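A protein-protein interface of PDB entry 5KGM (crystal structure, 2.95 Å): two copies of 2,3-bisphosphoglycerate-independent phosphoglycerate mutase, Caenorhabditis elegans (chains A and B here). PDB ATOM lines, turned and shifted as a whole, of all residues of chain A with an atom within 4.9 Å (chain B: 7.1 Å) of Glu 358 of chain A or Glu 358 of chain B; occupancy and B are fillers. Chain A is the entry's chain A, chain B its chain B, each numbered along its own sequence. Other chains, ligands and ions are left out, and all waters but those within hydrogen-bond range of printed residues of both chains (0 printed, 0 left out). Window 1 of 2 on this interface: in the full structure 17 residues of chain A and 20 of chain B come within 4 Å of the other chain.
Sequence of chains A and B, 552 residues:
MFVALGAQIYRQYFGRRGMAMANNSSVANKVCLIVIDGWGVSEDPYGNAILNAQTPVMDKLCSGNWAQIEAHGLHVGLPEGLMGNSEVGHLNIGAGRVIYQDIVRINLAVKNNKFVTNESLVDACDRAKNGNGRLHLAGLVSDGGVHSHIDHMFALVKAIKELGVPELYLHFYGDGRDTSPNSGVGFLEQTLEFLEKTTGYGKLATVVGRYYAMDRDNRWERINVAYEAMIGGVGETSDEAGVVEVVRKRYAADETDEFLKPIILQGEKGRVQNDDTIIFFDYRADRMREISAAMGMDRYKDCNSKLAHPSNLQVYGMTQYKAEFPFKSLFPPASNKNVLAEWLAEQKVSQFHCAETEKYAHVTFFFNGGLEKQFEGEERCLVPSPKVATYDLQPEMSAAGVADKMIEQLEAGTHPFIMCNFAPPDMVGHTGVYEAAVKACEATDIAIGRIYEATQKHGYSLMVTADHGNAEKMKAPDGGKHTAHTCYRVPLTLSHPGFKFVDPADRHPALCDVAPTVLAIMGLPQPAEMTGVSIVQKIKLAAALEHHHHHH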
ATOM      1  N   GLU A 356     -13.870   1.495 -39.671  1.00  0.00           N
ATOM      2  CA  GLU A 356     -12.842   1.082 -38.726  1.00  0.00           C
ATOM      3  C   GLU A 356     -13.480   0.356 -37.527  1.00  0.00           C
ATOM      4  O   GLU A 356     -14.703   0.340 -37.352  1.00  0.00           O
ATOM      5  CB  GLU A 356     -11.956   2.260 -38.310  1.00  0.00           C
ATOM      6  CG  GLU A 356     -12.500   3.251 -37.330  1.00  0.00           C
ATOM      7  CD  GLU A 356     -11.420   4.244 -36.921  1.00  0.00           C
ATOM      8  OE1 GLU A 356     -10.758   3.988 -35.897  1.00  0.00           O
ATOM      9  OE2 GLU A 356     -11.206   5.257 -37.634  1.00  0.00           O
ATOM     10  N   THR A 357     -12.620  -0.294 -36.730  1.00  0.00           N
ATOM     11  CA  THR A 357     -13.067  -1.277 -35.740  1.00  0.00           C
ATOM     12  C   THR A 357     -14.202  -0.774 -34.855  1.00  0.00           C
ATOM     13  O   THR A 357     -15.245  -1.430 -34.741  1.00  0.00           O
ATOM     14  CB  THR A 357     -11.887  -1.686 -34.860  1.00  0.00           C
ATOM     15  OG1 THR A 357     -10.793  -2.079 -35.696  1.00  0.00           O
ATOM     16  CG2 THR A 357     -12.277  -2.874 -33.947  1.00  0.00           C
ATOM     17  N   GLU A 358     -14.057   0.436 -34.295  1.00  0.00           N
ATOM     18  CA  GLU A 358     -15.031   0.931 -33.316  1.00  0.00           C
ATOM     19  C   GLU A 358     -16.432   1.050 -33.871  1.00  0.00           C
ATOM     20  O   GLU A 358     -17.383   1.138 -33.091  1.00  0.00           O
ATOM     21  CB  GLU A 358     -14.629   2.310 -32.790  1.00  0.00           C
ATOM     22  CG  GLU A 358     -13.382   2.354 -31.946  1.00  0.00           C
ATOM     23  CD  GLU A 358     -13.581   1.750 -30.558  1.00  0.00           C
ATOM     24  OE1 GLU A 358     -14.739   1.432 -30.175  1.00  0.00           O
ATOM     25  OE2 GLU A 358     -12.566   1.631 -29.835  1.00  0.00           O
ATOM     26  N   LYS A 359     -16.574   1.133 -35.186  1.00  0.00           N
ATOM     27  CA  LYS A 359     -17.876   1.269 -35.813  1.00  0.00           C
ATOM     28  C   LYS A 359     -18.118   0.156 -36.826  1.00  0.00           C
ATOM     29  O   LYS A 359     -19.051   0.240 -37.638  1.00  0.00           O
ATOM     30  CB  LYS A 359     -17.981   2.647 -36.466  1.00  0.00           C
ATOM     31  CG  LYS A 359     -17.868   3.817 -35.470  1.00  0.00           C
ATOM     32  CD  LYS A 359     -19.044   3.868 -34.484  1.00  0.00           C
ATOM     33  CE  LYS A 359     -18.896   4.993 -33.469  1.00  0.00           C
ATOM     34  NZ  LYS A 359     -20.112   5.110 -32.637  1.00  0.00           N
ATOM     35  N   TYR A 360     -17.316  -0.906 -36.778  1.00  0.00           N
ATOM     36  CA  TYR A 360     -17.479  -1.939 -37.788  1.00  0.00           C
ATOM     37  C   TYR A 360     -18.824  -2.643 -37.646  1.00  0.00           C
ATOM     38  O   TYR A 360     -19.578  -2.753 -38.623  1.00  0.00           O
ATOM     39  CB  TYR A 360     -16.306  -2.922 -37.718  1.00  0.00           C
ATOM     40  CG  TYR A 360     -16.375  -3.974 -38.794  1.00  0.00           C
ATOM     41  CD1 TYR A 360     -16.018  -3.646 -40.090  1.00  0.00           C
ATOM     42  CD2 TYR A 360     -16.783  -5.271 -38.537  1.00  0.00           C
ATOM     43  CE1 TYR A 360     -16.076  -4.568 -41.105  1.00  0.00           C
ATOM     44  CE2 TYR A 360     -16.847  -6.212 -39.556  1.00  0.00           C
ATOM     45  CZ  TYR A 360     -16.486  -5.853 -40.839  1.00  0.00           C
ATOM     46  OH  TYR A 360     -16.532  -6.759 -41.880  1.00  0.00           O
ATOM     47  N   HIS A 362     -21.453  -1.343 -36.650  1.00  0.00           N
ATOM     48  CA  HIS A 362     -22.513  -0.430 -37.042  1.00  0.00           C
ATOM     49  C   HIS A 362     -22.731  -0.435 -38.553  1.00  0.00           C
ATOM     50  O   HIS A 362     -23.878  -0.304 -39.002  1.00  0.00           O
ATOM     51  CB  HIS A 362     -22.178   0.951 -36.484  1.00  0.00           C
ATOM     52  CG  HIS A 362     -22.050   0.944 -34.994  1.00  0.00           C
ATOM     53  ND1 HIS A 362     -20.867   0.644 -34.349  1.00  0.00           N
ATOM     54  CD2 HIS A 362     -22.957   1.202 -34.019  1.00  0.00           C
ATOM     55  CE1 HIS A 362     -21.056   0.701 -33.041  1.00  0.00           C
ATOM     56  NE2 HIS A 362     -22.314   1.042 -32.815  1.00  0.00           N
ATOM     57  N   SER A 385      -8.543   0.316 -35.972  1.00  0.00           N
ATOM     58  CA  SER A 385      -8.411   1.552 -35.226  1.00  0.00           C
ATOM     59  C   SER A 385      -7.043   1.623 -34.550  1.00  0.00           C
ATOM     60  O   SER A 385      -6.440   0.594 -34.236  1.00  0.00           O
ATOM     61  CB  SER A 385      -9.514   1.656 -34.180  1.00  0.00           C
ATOM     62  OG  SER A 385     -10.762   1.898 -34.796  1.00  0.00           O
ATOM     63  N   TYR A 391      -8.724   8.005 -27.361  1.00  0.00           N
ATOM     64  CA  TYR A 391      -8.578   8.481 -28.736  1.00  0.00           C
ATOM     65  C   TYR A 391      -8.228   9.963 -28.852  1.00  0.00           C
ATOM     66  O   TYR A 391      -7.810  10.392 -29.936  1.00  0.00           O
ATOM     67  CB  TYR A 391      -9.837   8.157 -29.548  1.00  0.00           C
ATOM     68  CG  TYR A 391     -10.001   6.669 -29.797  1.00  0.00           C
ATOM     69  CD1 TYR A 391      -9.034   5.953 -30.494  1.00  0.00           C
ATOM     70  CD2 TYR A 391     -11.109   5.980 -29.328  1.00  0.00           C
ATOM     71  CE1 TYR A 391      -9.167   4.594 -30.710  1.00  0.00           C
ATOM     72  CE2 TYR A 391     -11.254   4.624 -29.549  1.00  0.00           C
ATOM     73  CZ  TYR A 391     -10.282   3.937 -30.234  1.00  0.00           C
ATOM     74  OH  TYR A 391     -10.437   2.587 -30.452  1.00  0.00           O
ATOM     75  N   MET A 397      -7.826   9.270 -35.603  1.00  0.00           N
ATOM     76  CA  MET A 397      -8.064   7.829 -35.625  1.00  0.00           C
ATOM     77  C   MET A 397      -7.598   7.171 -36.925  1.00  0.00           C
ATOM     78  O   MET A 397      -6.445   7.361 -37.329  1.00  0.00           O
ATOM     79  CB  MET A 397      -9.545   7.563 -35.318  1.00  0.00           C
ATOM     80  CG  MET A 397      -9.913   8.153 -33.955  1.00  0.00           C
ATOM     81  SD  MET A 397     -11.582   7.898 -33.354  1.00  0.00           S
ATOM     82  CE  MET A 397     -11.548   6.142 -33.065  1.00  0.00           C
ATOM     83  N   MET A 427     -16.174   9.337 -31.378  1.00  0.00           N
ATOM     84  CA  MET A 427     -15.332   8.662 -30.395  1.00  0.00           C
ATOM     85  C   MET A 427     -14.438   9.652 -29.669  1.00  0.00           C
ATOM     86  O   MET A 427     -14.219   9.524 -28.457  1.00  0.00           O
ATOM     87  CB  MET A 427     -14.476   7.579 -31.062  1.00  0.00           C
ATOM     88  CG  MET A 427     -15.236   6.418 -31.702  1.00  0.00           C
ATOM     89  SD  MET A 427     -16.355   5.631 -30.550  1.00  0.00           S
ATOM     90  CE  MET A 427     -15.180   4.895 -29.418  1.00  0.00           C
ATOM     91  N   ASP B  37     -12.254  -9.247 -20.773  1.00  0.00           N
ATOM     92  CA  ASP B  37     -11.481  -8.202 -21.436  1.00  0.00           C
ATOM     93  C   ASP B  37     -10.822  -7.272 -20.423  1.00  0.00           C
ATOM     94  O   ASP B  37     -11.516  -6.557 -19.696  1.00  0.00           O
ATOM     95  CB  ASP B  37     -12.364  -7.400 -22.384  1.00  0.00           C
ATOM     96  CG  ASP B  37     -11.608  -6.895 -23.579  1.00  0.00           C
ATOM     97  OD1 ASP B  37     -12.035  -7.188 -24.717  1.00  0.00           O
ATOM     98  OD2 ASP B  37     -10.586  -6.198 -23.371  1.00  0.00           O
ATOM     99  N   SER B  86      -7.036  -5.808 -27.620  1.00  0.00           N
ATOM    100  CA  SER B  86      -8.192  -6.677 -27.837  1.00  0.00           C
ATOM    101  C   SER B  86      -8.095  -7.419 -29.168  1.00  0.00           C
ATOM    102  O   SER B  86      -8.448  -8.604 -29.253  1.00  0.00           O
ATOM    103  CB  SER B  86      -9.484  -5.850 -27.773  1.00  0.00           C
ATOM    104  OG  SER B  86      -9.604  -5.164 -26.532  1.00  0.00           O
ATOM    105  N   GLU B  87      -7.566  -6.767 -30.203  1.00  0.00           N
ATOM    106  CA  GLU B  87      -7.541  -7.386 -31.523  1.00  0.00           C
ATOM    107  C   GLU B  87      -6.506  -8.500 -31.567  1.00  0.00           C
ATOM    108  O   GLU B  87      -6.808  -9.640 -31.960  1.00  0.00           O
ATOM    109  CB  GLU B  87      -7.229  -6.334 -32.585  1.00  0.00           C
ATOM    110  CG  GLU B  87      -8.278  -5.243 -32.756  1.00  0.00           C
ATOM    111  CD  GLU B  87      -7.887  -4.278 -33.876  1.00  0.00           C
ATOM    112  OE1 GLU B  87      -7.064  -4.673 -34.736  1.00  0.00           O
ATOM    113  OE2 GLU B  87      -8.385  -3.131 -33.904  1.00  0.00           O
ATOM    114  N   ALA B 355     -21.053 -11.779 -27.565  1.00  0.00           N
ATOM    115  CA  ALA B 355     -20.468 -10.611 -26.920  1.00  0.00           C
ATOM    116  C   ALA B 355     -21.482  -9.482 -26.983  1.00  0.00           C
ATOM    117  O   ALA B 355     -22.496  -9.578 -27.677  1.00  0.00           O
ATOM    118  CB  ALA B 355     -19.147 -10.211 -27.573  1.00  0.00           C
ATOM    119  N   GLU B 356     -21.244  -8.443 -26.186  1.00  0.00           N
ATOM    120  CA  GLU B 356     -21.962  -7.198 -26.390  1.00  0.00           C
ATOM    121  C   GLU B 356     -21.241  -6.349 -27.446  1.00  0.00           C
ATOM    122  O   GLU B 356     -20.148  -6.683 -27.913  1.00  0.00           O
ATOM    123  CB  GLU B 356     -22.148  -6.445 -25.068  1.00  0.00           C
ATOM    124  CG  GLU B 356     -20.921  -5.776 -24.462  1.00  0.00           C
ATOM    125  CD  GLU B 356     -21.243  -5.038 -23.150  1.00  0.00           C
ATOM    126  OE1 GLU B 356     -21.426  -3.799 -23.193  1.00  0.00           O
ATOM    127  OE2 GLU B 356     -21.314  -5.696 -22.081  1.00  0.00           O
ATOM    128  N   THR B 357     -21.890  -5.252 -27.843  1.00  0.00           N
ATOM    129  CA  THR B 357     -21.479  -4.504 -29.034  1.00  0.00           C
ATOM    130  C   THR B 357     -19.998  -4.099 -29.043  1.00  0.00           C
ATOM    131  O   THR B 357     -19.312  -4.275 -30.057  1.00  0.00           O
ATOM    132  CB  THR B 357     -22.371  -3.275 -29.209  1.00  0.00           C
ATOM    133  OG1 THR B 357     -23.748  -3.664 -29.124  1.00  0.00           O
ATOM    134  CG2 THR B 357     -22.117  -2.638 -30.553  1.00  0.00           C
ATOM    135  N   GLU B 358     -19.476  -3.562 -27.929  1.00  0.00           N
ATOM    136  CA  GLU B 358     -18.108  -3.031 -27.952  1.00  0.00           C
ATOM    137  C   GLU B 358     -17.053  -4.076 -28.264  1.00  0.00           C
ATOM    138  O   GLU B 358     -15.944  -3.706 -28.671  1.00  0.00           O
ATOM    139  CB  GLU B 358     -17.749  -2.367 -26.625  1.00  0.00           C
ATOM    140  CG  GLU B 358     -18.484  -1.080 -26.331  1.00  0.00           C
ATOM    141  CD  GLU B 358     -18.005   0.086 -27.193  1.00  0.00           C
ATOM    142  OE1 GLU B 358     -16.954  -0.037 -27.878  1.00  0.00           O
ATOM    143  OE2 GLU B 358     -18.674   1.141 -27.155  1.00  0.00           O
ATOM    144  N   LYS B 359     -17.329  -5.355 -28.026  1.00  0.00           N
ATOM    145  CA  LYS B 359     -16.351  -6.405 -28.292  1.00  0.00           C
ATOM    146  C   LYS B 359     -16.932  -7.435 -29.257  1.00  0.00           C
ATOM    147  O   LYS B 359     -16.409  -8.548 -29.371  1.00  0.00           O
ATOM    148  CB  LYS B 359     -15.899  -7.080 -26.991  1.00  0.00           C
ATOM    149  CG  LYS B 359     -15.256  -6.110 -25.970  1.00  0.00           C
ATOM    150  CD  LYS B 359     -13.932  -5.499 -26.445  1.00  0.00           C
ATOM    151  CE  LYS B 359     -13.362  -4.527 -25.411  1.00  0.00           C
ATOM    152  NZ  LYS B 359     -12.010  -4.033 -25.782  1.00  0.00           N
ATOM    153  N   TYR B 360     -18.019  -7.089 -29.945  1.00  0.00           N
ATOM    154  CA  TYR B 360     -18.654  -8.053 -30.832  1.00  0.00           C
ATOM    155  C   TYR B 360     -17.761  -8.384 -32.019  1.00  0.00           C
ATOM    156  O   TYR B 360     -17.739  -9.533 -32.480  1.00  0.00           O
ATOM    157  CB  TYR B 360     -20.001  -7.524 -31.314  1.00  0.00           C
ATOM    158  CG  TYR B 360     -20.718  -8.503 -32.197  1.00  0.00           C
ATOM    159  CD1 TYR B 360     -21.321  -9.615 -31.620  1.00  0.00           C
ATOM    160  CD2 TYR B 360     -20.809  -8.343 -33.568  1.00  0.00           C
ATOM    161  CE1 TYR B 360     -21.993 -10.543 -32.370  1.00  0.00           C
ATOM    162  CE2 TYR B 360     -21.493  -9.284 -34.345  1.00  0.00           C
ATOM    163  CZ  TYR B 360     -22.089 -10.380 -33.726  1.00  0.00           C
ATOM    164  OH  TYR B 360     -22.783 -11.344 -34.430  1.00  0.00           O
ATOM    165  N   ALA B 361     -17.076  -7.376 -32.577  1.00  0.00           N
ATOM    166  CA  ALA B 361     -16.119  -7.632 -33.657  1.00  0.00           C
ATOM    167  C   ALA B 361     -14.980  -8.540 -33.211  1.00  0.00           C
ATOM    168  O   ALA B 361     -14.474  -9.338 -34.003  1.00  0.00           O
ATOM    169  CB  ALA B 361     -15.532  -6.319 -34.159  1.00  0.00           C
ATOM    170  N   HIS B 362     -14.575  -8.444 -31.947  1.00  0.00           N
ATOM    171  CA  HIS B 362     -13.433  -9.205 -31.470  1.00  0.00           C
ATOM    172  C   HIS B 362     -13.734 -10.697 -31.371  1.00  0.00           C
ATOM    173  O   HIS B 362     -12.865 -11.526 -31.670  1.00  0.00           O
ATOM    174  CB  HIS B 362     -12.997  -8.622 -30.130  1.00  0.00           C
ATOM    175  CG  HIS B 362     -12.652  -7.171 -30.221  1.00  0.00           C
ATOM    176  ND1 HIS B 362     -13.610  -6.183 -30.198  1.00  0.00           N
ATOM    177  CD2 HIS B 362     -11.460  -6.539 -30.349  1.00  0.00           C
ATOM    178  CE1 HIS B 362     -13.024  -5.003 -30.308  1.00  0.00           C
ATOM    179  NE2 HIS B 362     -11.719  -5.190 -30.401  1.00  0.00           N
ATOM    180  N   LEU B 382     -25.254 -11.086 -30.320  1.00  0.00           N
ATOM    181  CA  LEU B 382     -24.822  -9.744 -29.938  1.00  0.00           C
ATOM    182  C   LEU B 382     -25.801  -9.184 -28.915  1.00  0.00           C
ATOM    183  O   LEU B 382     -27.017  -9.218 -29.122  1.00  0.00           O
ATOM    184  CB  LEU B 382     -24.729  -8.792 -31.135  1.00  0.00           C
ATOM    185  CG  LEU B 382     -24.534  -7.310 -30.775  1.00  0.00           C
ATOM    186  CD1 LEU B 382     -23.875  -6.645 -31.936  1.00  0.00           C
ATOM    187  CD2 LEU B 382     -25.814  -6.531 -30.432  1.00  0.00           C
ATOM    188  N   VAL B 383     -25.258  -8.678 -27.819  1.00  0.00           N
ATOM    189  CA  VAL B 383     -25.999  -7.984 -26.771  1.00  0.00           C
ATOM    190  C   VAL B 383     -25.715  -6.490 -26.873  1.00  0.00           C
ATOM    191  O   VAL B 383     -24.546  -6.092 -26.867  1.00  0.00           O
ATOM    192  CB  VAL B 383     -25.599  -8.512 -25.381  1.00  0.00           C
ATOM    193  CG1 VAL B 383     -26.296  -7.776 -24.289  1.00  0.00           C
ATOM    194  CG2 VAL B 383     -25.932  -9.997 -25.285  1.00  0.00           C
ATOM    195  N   PRO B 384     -26.735  -5.633 -26.952  1.00  0.00           N
ATOM    196  CA  PRO B 384     -26.476  -4.191 -27.050  1.00  0.00           C
ATOM    197  C   PRO B 384     -25.760  -3.656 -25.816  1.00  0.00           C
ATOM    198  O   PRO B 384     -26.040  -4.058 -24.682  1.00  0.00           O
ATOM    199  CB  PRO B 384     -27.873  -3.587 -27.201  1.00  0.00           C
ATOM    200  CG  PRO B 384     -28.694  -4.697 -27.738  1.00  0.00           C
ATOM    201  CD  PRO B 384     -28.166  -5.934 -27.134  1.00  0.00           C
ATOM    202  N   SER B 385     -24.756  -2.820 -26.057  1.00  0.00           N
ATOM    203  CA  SER B 385     -24.138  -2.060 -24.985  1.00  0.00           C
ATOM    204  C   SER B 385     -25.091  -0.963 -24.507  1.00  0.00           C
ATOM    205  O   SER B 385     -25.972  -0.521 -25.248  1.00  0.00           O
ATOM    206  CB  SER B 385     -22.816  -1.442 -25.451  1.00  0.00           C
ATOM    207  OG  SER B 385     -21.824  -2.428 -25.737  1.00  0.00           O
ATOM    208  N   PRO B 386     -24.938  -0.510 -23.267  1.00  0.00           N
ATOM    209  CA  PRO B 386     -25.799   0.561 -22.767  1.00  0.00           C
ATOM    210  C   PRO B 386     -25.547   1.866 -23.493  1.00  0.00           C
ATOM    211  O   PRO B 386     -24.455   2.117 -24.011  1.00  0.00           O
ATOM    212  CB  PRO B 386     -25.411   0.673 -21.288  1.00  0.00           C
ATOM    213  CG  PRO B 386     -24.071   0.112 -21.204  1.00  0.00           C
ATOM    214  CD  PRO B 386     -23.992  -0.967 -22.241  1.00  0.00           C
ATOM    215  N   TYR B 391     -18.770   4.928 -19.942  1.00  0.00           N
ATOM    216  CA  TYR B 391     -19.177   3.691 -19.272  1.00  0.00           C
ATOM    217  C   TYR B 391     -18.946   3.695 -17.761  1.00  0.00           C
ATOM    218  O   TYR B 391     -19.481   2.816 -17.072  1.00  0.00           O
ATOM    219  CB  TYR B 391     -18.480   2.494 -19.914  1.00  0.00           C
ATOM    220  CG  TYR B 391     -18.986   2.263 -21.321  1.00  0.00           C
ATOM    221  CD1 TYR B 391     -20.334   2.053 -21.572  1.00  0.00           C
ATOM    222  CD2 TYR B 391     -18.112   2.273 -22.404  1.00  0.00           C
ATOM    223  CE1 TYR B 391     -20.805   1.863 -22.863  1.00  0.00           C
ATOM    224  CE2 TYR B 391     -18.573   2.081 -23.699  1.00  0.00           C
ATOM    225  CZ  TYR B 391     -19.917   1.881 -23.924  1.00  0.00           C
ATOM    226  OH  TYR B 391     -20.369   1.689 -25.212  1.00  0.00           O
ATOM    227  N   MET B 397     -21.975  -2.274 -17.430  1.00  0.00           N
ATOM    228  CA  MET B 397     -22.317  -2.356 -18.843  1.00  0.00           C
ATOM    229  C   MET B 397     -23.437  -3.365 -19.107  1.00  0.00           C
ATOM    230  O   MET B 397     -24.491  -3.296 -18.464  1.00  0.00           O
ATOM    231  CB  MET B 397     -21.039  -2.671 -19.632  1.00  0.00           C
ATOM    232  CG  MET B 397     -19.957  -1.585 -19.431  1.00  0.00           C
ATOM    233  SD  MET B 397     -18.397  -1.780 -20.329  1.00  0.00           S
ATOM    234  CE  MET B 397     -18.946  -1.563 -22.024  1.00  0.00           C
ATOM    235  N   ASN B 421     -17.334 -12.997 -24.583  1.00  0.00           N
ATOM    236  CA  ASN B 421     -16.469 -11.929 -24.076  1.00  0.00           C
ATOM    237  C   ASN B 421     -17.204 -11.134 -22.998  1.00  0.00           C
ATOM    238  O   ASN B 421     -18.420 -10.938 -23.085  1.00  0.00           O
ATOM    239  CB  ASN B 421     -16.047 -10.990 -25.222  1.00  0.00           C
ATOM    240  CG  ASN B 421     -15.260  -9.768 -24.746  1.00  0.00           C
ATOM    241  OD1 ASN B 421     -15.808  -8.859 -24.116  1.00  0.00           O
ATOM    242  ND2 ASN B 421     -13.974  -9.730 -25.074  1.00  0.00           N
ATOM    243  N   ALA B 423     -16.856  -7.343 -21.347  1.00  0.00           N
ATOM    244  CA  ALA B 423     -16.275  -6.034 -21.666  1.00  0.00           C
ATOM    245  C   ALA B 423     -15.865  -5.101 -20.520  1.00  0.00           C
ATOM    246  O   ALA B 423     -14.935  -4.307 -20.699  1.00  0.00           O
ATOM    247  CB  ALA B 423     -17.275  -5.261 -22.530  1.00  0.00           C
ATOM    248  N   MET B 427     -13.205  -1.537 -20.918  1.00  0.00           N
ATOM    249  CA  MET B 427     -13.870  -0.314 -21.342  1.00  0.00           C
ATOM    250  C   MET B 427     -13.985   0.677 -20.192  1.00  0.00           C
ATOM    251  O   MET B 427     -13.775   1.880 -20.385  1.00  0.00           O
ATOM    252  CB  MET B 427     -15.241  -0.659 -21.921  1.00  0.00           C
ATOM    253  CG  MET B 427     -15.194  -1.614 -23.128  1.00  0.00           C
ATOM    254  SD  MET B 427     -14.143  -1.017 -24.464  1.00  0.00           S
ATOM    255  CE  MET B 427     -15.004   0.478 -24.958  1.00  0.00           C
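Glu 358 of chain B touches its own counterpart, Glu 358 of chain A.
10 positions are printed for both chains.
Of the 2 pairs that touch across the chains among the printed residues, 1 has its exchanged pair printed and touching as well.
OG1 of Thr 357 of chain A sits at hydrogen-bond distance from OE2 of Glu 87 of chain B (3.2 Å).
Of the printed residues of chain B, Thr 357 of chain A touches Glu 87.
Of chain B, only Glu 358 (3.5 Å) comes within 4 Å of Glu 358 of chain A.
Of the printed residues of chain A, Glu 87 of chain B touches Thr 357.
Of chain A, only Glu 358 comes within 4 Å of Glu 358 of chain B.
Pro 386 of chain B touches none of the printed residues of chain A.
Among the printed residues, no Asp or Glu carboxylate lies within 4 Å of a Lys or Arg side-chain nitrogen of the other chain.
Among the printed residues, pairs that only touch across the chains: Glu 358 of chain A with Glu 358 of chain B.
The side-chain hydroxyl (OG1) of Thr 357 of chain A sits at hydrogen-bond distance from the backbone NH (N) of Ser 385 of chain A, 3.3 Å away.
The side-chain carboxylate of Glu 358 of chain A sits at hydrogen-bond distance from the side-chain hydroxyl of Tyr 391 of chain A (2.4 Å).
OG of Ser 385 of chain B lies within hydrogen-bond range of N of Glu 358 of chain B (3.4 Å).
OH of Tyr 391 of chain B lies within hydrogen-bond range of OE2 of Glu 358 of chain B, at 2.6 Å.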
